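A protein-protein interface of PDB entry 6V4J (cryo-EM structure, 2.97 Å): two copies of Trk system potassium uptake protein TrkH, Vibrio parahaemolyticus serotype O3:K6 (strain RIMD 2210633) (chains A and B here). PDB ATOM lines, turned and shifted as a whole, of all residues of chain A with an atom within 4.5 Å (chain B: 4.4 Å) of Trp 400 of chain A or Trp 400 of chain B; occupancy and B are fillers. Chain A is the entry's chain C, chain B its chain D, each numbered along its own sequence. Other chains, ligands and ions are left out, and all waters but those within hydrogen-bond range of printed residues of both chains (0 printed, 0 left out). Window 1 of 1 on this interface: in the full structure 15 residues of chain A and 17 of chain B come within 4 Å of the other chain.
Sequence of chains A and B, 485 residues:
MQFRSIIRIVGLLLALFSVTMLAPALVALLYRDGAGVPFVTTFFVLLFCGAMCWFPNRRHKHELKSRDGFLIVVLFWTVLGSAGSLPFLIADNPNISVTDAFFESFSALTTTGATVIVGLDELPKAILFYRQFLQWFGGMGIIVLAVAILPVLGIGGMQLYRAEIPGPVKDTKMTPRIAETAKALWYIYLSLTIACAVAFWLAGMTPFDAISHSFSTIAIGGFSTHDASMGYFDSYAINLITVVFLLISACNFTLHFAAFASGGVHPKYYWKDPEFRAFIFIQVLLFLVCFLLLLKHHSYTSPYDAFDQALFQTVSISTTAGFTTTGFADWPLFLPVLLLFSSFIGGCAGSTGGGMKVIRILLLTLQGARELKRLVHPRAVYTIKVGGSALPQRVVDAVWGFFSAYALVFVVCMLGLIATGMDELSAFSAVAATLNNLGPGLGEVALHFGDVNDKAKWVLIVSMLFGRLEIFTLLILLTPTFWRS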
ATOM      1  N   LEU A 364     -13.684  36.237   6.317  1.00  0.00           N
ATOM      2  CA  LEU A 364     -14.920  35.792   6.951  1.00  0.00           C
ATOM      3  C   LEU A 364     -16.125  36.580   6.465  1.00  0.00           C
ATOM      4  O   LEU A 364     -17.191  36.016   6.259  1.00  0.00           O
ATOM      5  CB  LEU A 364     -14.815  35.910   8.461  1.00  0.00           C
ATOM      6  CG  LEU A 364     -14.027  34.811   9.139  1.00  0.00           C
ATOM      7  CD1 LEU A 364     -13.790  35.197  10.589  1.00  0.00           C
ATOM      8  CD2 LEU A 364     -14.797  33.519   9.041  1.00  0.00           C
ATOM      9  N   GLN A 367     -16.214  36.204   2.405  1.00  0.00           N
ATOM     10  CA  GLN A 367     -16.488  34.796   2.162  1.00  0.00           C
ATOM     11  C   GLN A 367     -17.770  34.485   2.887  1.00  0.00           C
ATOM     12  O   GLN A 367     -18.417  33.466   2.649  1.00  0.00           O
ATOM     13  CB  GLN A 367     -15.352  33.833   2.535  1.00  0.00           C
ATOM     14  CG  GLN A 367     -13.970  33.805   1.804  1.00  0.00           C
ATOM     15  CD  GLN A 367     -13.940  33.873   0.294  1.00  0.00           C
ATOM     16  OE1 GLN A 367     -14.946  33.799  -0.395  1.00  0.00           O
ATOM     17  NE2 GLN A 367     -12.734  33.974  -0.231  1.00  0.00           N
ATOM     18  N   VAL A 396      -8.056  28.474   3.245  1.00  0.00           N
ATOM     19  CA  VAL A 396      -9.113  29.342   3.727  1.00  0.00           C
ATOM     20  C   VAL A 396      -9.773  28.687   4.910  1.00  0.00           C
ATOM     21  O   VAL A 396     -10.157  29.365   5.865  1.00  0.00           O
ATOM     22  CB  VAL A 396     -10.098  29.702   2.580  1.00  0.00           C
ATOM     23  CG1 VAL A 396     -10.877  28.527   2.044  1.00  0.00           C
ATOM     24  CG2 VAL A 396     -11.125  30.701   3.045  1.00  0.00           C
ATOM     25  N   ASP A 397      -9.887  27.360   4.859  1.00  0.00           N
ATOM     26  CA  ASP A 397     -10.464  26.619   5.956  1.00  0.00           C
ATOM     27  C   ASP A 397      -9.596  26.801   7.182  1.00  0.00           C
ATOM     28  O   ASP A 397     -10.092  26.949   8.299  1.00  0.00           O
ATOM     29  CB  ASP A 397     -10.567  25.156   5.557  1.00  0.00           C
ATOM     30  CG  ASP A 397     -11.685  24.910   4.574  1.00  0.00           C
ATOM     31  OD1 ASP A 397     -12.469  25.842   4.335  1.00  0.00           O
ATOM     32  OD2 ASP A 397     -11.773  23.790   4.026  1.00  0.00           O
ATOM     33  N   ALA A 398      -8.286  26.843   6.955  1.00  0.00           N
ATOM     34  CA  ALA A 398      -7.314  27.052   8.010  1.00  0.00           C
ATOM     35  C   ALA A 398      -7.495  28.394   8.687  1.00  0.00           C
ATOM     36  O   ALA A 398      -7.192  28.517   9.874  1.00  0.00           O
ATOM     37  CB  ALA A 398      -5.896  26.914   7.462  1.00  0.00           C
ATOM     38  N   VAL A 399      -7.803  29.443   7.919  1.00  0.00           N
ATOM     39  CA  VAL A 399      -7.950  30.756   8.553  1.00  0.00           C
ATOM     40  C   VAL A 399      -9.098  30.774   9.550  1.00  0.00           C
ATOM     41  O   VAL A 399      -8.950  31.247  10.681  1.00  0.00           O
ATOM     42  CB  VAL A 399      -8.121  31.867   7.505  1.00  0.00           C
ATOM     43  CG1 VAL A 399      -7.960  33.214   8.179  1.00  0.00           C
ATOM     44  CG2 VAL A 399      -7.094  31.753   6.415  1.00  0.00           C
ATOM     45  N   TRP A 400     -10.268  30.308   9.144  1.00  0.00           N
ATOM     46  CA  TRP A 400     -11.364  30.303  10.103  1.00  0.00           C
ATOM     47  C   TRP A 400     -11.170  29.244  11.177  1.00  0.00           C
ATOM     48  O   TRP A 400     -11.742  29.360  12.263  1.00  0.00           O
ATOM     49  CB  TRP A 400     -12.722  30.330   9.411  1.00  0.00           C
ATOM     50  CG  TRP A 400     -13.016  29.336   8.437  1.00  0.00           C
ATOM     51  CD1 TRP A 400     -12.954  27.990   8.566  1.00  0.00           C
ATOM     52  CD2 TRP A 400     -13.609  29.595   7.166  1.00  0.00           C
ATOM     53  NE1 TRP A 400     -13.367  27.391   7.406  1.00  0.00           N
ATOM     54  CE2 TRP A 400     -13.804  28.359   6.542  1.00  0.00           C
ATOM     55  CE3 TRP A 400     -13.966  30.760   6.486  1.00  0.00           C
ATOM     56  CZ2 TRP A 400     -14.341  28.252   5.270  1.00  0.00           C
ATOM     57  CZ3 TRP A 400     -14.502  30.649   5.233  1.00  0.00           C
ATOM     58  CH2 TRP A 400     -14.678  29.410   4.633  1.00  0.00           C
ATOM     59  N   GLY A 401     -10.466  28.168  10.858  1.00  0.00           N
ATOM     60  CA  GLY A 401     -10.147  27.170  11.866  1.00  0.00           C
ATOM     61  C   GLY A 401      -9.254  27.780  12.920  1.00  0.00           C
ATOM     62  O   GLY A 401      -9.331  27.441  14.100  1.00  0.00           O
ATOM     63  N   PHE A 402      -8.338  28.625  12.468  1.00  0.00           N
ATOM     64  CA  PHE A 402      -7.427  29.378  13.311  1.00  0.00           C
ATOM     65  C   PHE A 402      -8.221  30.302  14.201  1.00  0.00           C
ATOM     66  O   PHE A 402      -7.862  30.519  15.363  1.00  0.00           O
ATOM     67  CB  PHE A 402      -6.513  30.172  12.374  1.00  0.00           C
ATOM     68  CG  PHE A 402      -5.660  31.207  13.027  1.00  0.00           C
ATOM     69  CD1 PHE A 402      -4.597  30.882  13.820  1.00  0.00           C
ATOM     70  CD2 PHE A 402      -5.979  32.543  12.856  1.00  0.00           C
ATOM     71  CE1 PHE A 402      -3.832  31.877  14.402  1.00  0.00           C
ATOM     72  CE2 PHE A 402      -5.237  33.525  13.451  1.00  0.00           C
ATOM     73  CZ  PHE A 402      -4.160  33.192  14.220  1.00  0.00           C
ATOM     74  N   PHE A 403      -9.247  30.930  13.632  1.00  0.00           N
ATOM     75  CA  PHE A 403     -10.129  31.778  14.415  1.00  0.00           C
ATOM     76  C   PHE A 403     -10.893  30.956  15.454  1.00  0.00           C
ATOM     77  O   PHE A 403     -11.099  31.409  16.580  1.00  0.00           O
ATOM     78  CB  PHE A 403     -11.084  32.507  13.469  1.00  0.00           C
ATOM     79  CG  PHE A 403     -12.112  33.374  14.151  1.00  0.00           C
ATOM     80  CD1 PHE A 403     -11.787  34.156  15.249  1.00  0.00           C
ATOM     81  CD2 PHE A 403     -13.414  33.402  13.696  1.00  0.00           C
ATOM     82  CE1 PHE A 403     -12.744  34.947  15.868  1.00  0.00           C
ATOM     83  CE2 PHE A 403     -14.374  34.195  14.320  1.00  0.00           C
ATOM     84  CZ  PHE A 403     -14.033  34.968  15.402  1.00  0.00           C
ATOM     85  N   SER A 404     -11.363  29.763  15.079  1.00  0.00           N
ATOM     86  CA  SER A 404     -12.095  28.940  16.039  1.00  0.00           C
ATOM     87  C   SER A 404     -11.215  28.508  17.196  1.00  0.00           C
ATOM     88  O   SER A 404     -11.599  28.632  18.370  1.00  0.00           O
ATOM     89  CB  SER A 404     -12.668  27.725  15.329  1.00  0.00           C
ATOM     90  OG  SER A 404     -11.656  26.762  15.131  1.00  0.00           O
ATOM     91  N   LEU B 364     -16.580  21.475  15.165  1.00  0.00           N
ATOM     92  CA  LEU B 364     -15.474  22.414  15.344  1.00  0.00           C
ATOM     93  C   LEU B 364     -14.309  21.777  16.083  1.00  0.00           C
ATOM     94  O   LEU B 364     -13.155  21.980  15.724  1.00  0.00           O
ATOM     95  CB  LEU B 364     -15.946  23.639  16.096  1.00  0.00           C
ATOM     96  CG  LEU B 364     -16.707  24.620  15.236  1.00  0.00           C
ATOM     97  CD1 LEU B 364     -17.298  25.670  16.148  1.00  0.00           C
ATOM     98  CD2 LEU B 364     -15.776  25.231  14.212  1.00  0.00           C
ATOM     99  N   GLN B 367     -13.370  18.166  14.096  1.00  0.00           N
ATOM    100  CA  GLN B 367     -12.934  18.671  12.800  1.00  0.00           C
ATOM    101  C   GLN B 367     -11.763  19.586  13.043  1.00  0.00           C
ATOM    102  O   GLN B 367     -10.928  19.807  12.164  1.00  0.00           O
ATOM    103  CB  GLN B 367     -14.049  19.337  12.003  1.00  0.00           C
ATOM    104  CG  GLN B 367     -15.085  18.432  11.319  1.00  0.00           C
ATOM    105  CD  GLN B 367     -14.501  17.312  10.548  1.00  0.00           C
ATOM    106  OE1 GLN B 367     -13.573  17.510   9.789  1.00  0.00           O
ATOM    107  NE2 GLN B 367     -15.041  16.124  10.718  1.00  0.00           N
ATOM    108  N   VAL B 396     -20.485  21.234   6.381  1.00  0.00           N
ATOM    109  CA  VAL B 396     -19.608  21.610   7.495  1.00  0.00           C
ATOM    110  C   VAL B 396     -19.193  23.065   7.386  1.00  0.00           C
ATOM    111  O   VAL B 396     -19.291  23.832   8.354  1.00  0.00           O
ATOM    112  CB  VAL B 396     -18.405  20.658   7.596  1.00  0.00           C
ATOM    113  CG1 VAL B 396     -18.015  20.170   6.264  1.00  0.00           C
ATOM    114  CG2 VAL B 396     -17.222  21.327   8.246  1.00  0.00           C
ATOM    115  N   ASP B 397     -18.817  23.467   6.175  1.00  0.00           N
ATOM    116  CA  ASP B 397     -18.399  24.829   5.933  1.00  0.00           C
ATOM    117  C   ASP B 397     -19.552  25.766   6.201  1.00  0.00           C
ATOM    118  O   ASP B 397     -19.374  26.804   6.849  1.00  0.00           O
ATOM    119  CB  ASP B 397     -17.867  24.949   4.514  1.00  0.00           C
ATOM    120  CG  ASP B 397     -16.580  24.184   4.328  1.00  0.00           C
ATOM    121  OD1 ASP B 397     -16.156  23.533   5.293  1.00  0.00           O
ATOM    122  OD2 ASP B 397     -16.031  24.167   3.211  1.00  0.00           O
ATOM    123  N   ALA B 398     -20.743  25.385   5.743  1.00  0.00           N
ATOM    124  CA  ALA B 398     -21.924  26.197   5.987  1.00  0.00           C
ATOM    125  C   ALA B 398     -22.190  26.356   7.481  1.00  0.00           C
ATOM    126  O   ALA B 398     -22.568  27.439   7.935  1.00  0.00           O
ATOM    127  CB  ALA B 398     -23.139  25.587   5.284  1.00  0.00           C
ATOM    128  N   VAL B 399     -22.035  25.273   8.249  1.00  0.00           N
ATOM    129  CA  VAL B 399     -22.284  25.310   9.689  1.00  0.00           C
ATOM    130  C   VAL B 399     -21.326  26.233  10.422  1.00  0.00           C
ATOM    131  O   VAL B 399     -21.752  27.058  11.242  1.00  0.00           O
ATOM    132  CB  VAL B 399     -22.224  23.879  10.261  1.00  0.00           C
ATOM    133  CG1 VAL B 399     -22.090  23.887  11.769  1.00  0.00           C
ATOM    134  CG2 VAL B 399     -23.492  23.117   9.893  1.00  0.00           C
ATOM    135  N   TRP B 400     -20.027  26.121  10.161  1.00  0.00           N
ATOM    136  CA  TRP B 400     -19.129  27.032  10.874  1.00  0.00           C
ATOM    137  C   TRP B 400     -19.271  28.462  10.383  1.00  0.00           C
ATOM    138  O   TRP B 400     -18.969  29.403  11.125  1.00  0.00           O
ATOM    139  CB  TRP B 400     -17.698  26.514  10.969  1.00  0.00           C
ATOM    140  CG  TRP B 400     -16.976  26.158   9.796  1.00  0.00           C
ATOM    141  CD1 TRP B 400     -16.858  26.860   8.645  1.00  0.00           C
ATOM    142  CD2 TRP B 400     -16.059  25.068   9.702  1.00  0.00           C
ATOM    143  NE1 TRP B 400     -16.017  26.208   7.786  1.00  0.00           N
ATOM    144  CE2 TRP B 400     -15.491  25.116   8.424  1.00  0.00           C
ATOM    145  CE3 TRP B 400     -15.693  24.034  10.564  1.00  0.00           C
ATOM    146  CZ2 TRP B 400     -14.578  24.173   7.988  1.00  0.00           C
ATOM    147  CZ3 TRP B 400     -14.782  23.107  10.130  1.00  0.00           C
ATOM    148  CH2 TRP B 400     -14.235  23.180   8.857  1.00  0.00           C
ATOM    149  N   GLY B 401     -19.640  28.637   9.122  1.00  0.00           N
ATOM    150  CA  GLY B 401     -19.917  29.971   8.617  1.00  0.00           C
ATOM    151  C   GLY B 401     -21.086  30.566   9.369  1.00  0.00           C
ATOM    152  O   GLY B 401     -21.130  31.772   9.628  1.00  0.00           O
ATOM    153  N   PHE B 402     -22.076  29.725   9.660  1.00  0.00           N
ATOM    154  CA  PHE B 402     -23.237  30.106  10.448  1.00  0.00           C
ATOM    155  C   PHE B 402     -22.787  30.538  11.825  1.00  0.00           C
ATOM    156  O   PHE B 402     -23.362  31.460  12.413  1.00  0.00           O
ATOM    157  CB  PHE B 402     -24.204  28.919  10.503  1.00  0.00           C
ATOM    158  CG  PHE B 402     -25.214  28.963  11.617  1.00  0.00           C
ATOM    159  CD1 PHE B 402     -26.348  29.746  11.535  1.00  0.00           C
ATOM    160  CD2 PHE B 402     -25.041  28.160  12.732  1.00  0.00           C
ATOM    161  CE1 PHE B 402     -27.271  29.759  12.566  1.00  0.00           C
ATOM    162  CE2 PHE B 402     -25.958  28.165  13.764  1.00  0.00           C
ATOM    163  CZ  PHE B 402     -27.073  28.960  13.679  1.00  0.00           C
ATOM    164  N   PHE B 403     -21.828  29.812  12.393  1.00  0.00           N
ATOM    165  CA  PHE B 403     -21.287  30.199  13.685  1.00  0.00           C
ATOM    166  C   PHE B 403     -20.580  31.555  13.589  1.00  0.00           C
ATOM    167  O   PHE B 403     -20.666  32.369  14.508  1.00  0.00           O
ATOM    168  CB  PHE B 403     -20.335  29.112  14.182  1.00  0.00           C
ATOM    169  CG  PHE B 403     -19.604  29.432  15.471  1.00  0.00           C
ATOM    170  CD1 PHE B 403     -20.216  30.106  16.523  1.00  0.00           C
ATOM    171  CD2 PHE B 403     -18.297  29.037  15.636  1.00  0.00           C
ATOM    172  CE1 PHE B 403     -19.528  30.385  17.693  1.00  0.00           C
ATOM    173  CE2 PHE B 403     -17.609  29.313  16.813  1.00  0.00           C
ATOM    174  CZ  PHE B 403     -18.229  29.984  17.836  1.00  0.00           C
ATOM    175  N   SER B 404     -19.842  31.804  12.505  1.00  0.00           N
ATOM    176  CA  SER B 404     -19.166  33.094  12.390  1.00  0.00           C
ATOM    177  C   SER B 404     -20.156  34.244  12.321  1.00  0.00           C
ATOM    178  O   SER B 404     -20.018  35.243  13.044  1.00  0.00           O
ATOM    179  CB  SER B 404     -18.274  33.078  11.156  1.00  0.00           C
ATOM    180  OG  SER B 404     -19.070  33.204   9.997  1.00  0.00           O
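Trp 400 of chain A touches just one residue of chain B: Trp 400 (2.9 Å).
The nearest printed residue of chain B that does not touch Trp 400 of chain A is Asp 397 of chain B (4.7 Å).
The nearest printed residue of chain A that does not touch Trp 400 of chain B is Asp 397 of chain A (4.5 Å).
Printed residues of chain B that touch a printed residue of chain A: Trp 400.
Hydrophobic or aromatic side chains of chain B that line the printed part of chain A: Trp 400.
Of the 11 printed residues of chain A, 1 touches a printed residue of chain B.
Hydrophobic or aromatic side chains of chain A within 4 Å of the printed part of chain B: Trp 400.
The backbone carbonyl oxygen (O) of Asp 397 of chain A sits close to the indole nitrogen (NE1) of Trp 400 of chain A, at 3.4 Å.
Trp 400 of chain B touches its own counterpart, Trp 400 of chain A.
NE1 of Trp 400 of chain A sits close to NE1 of Trp 400 of chain B (2.9 Å).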
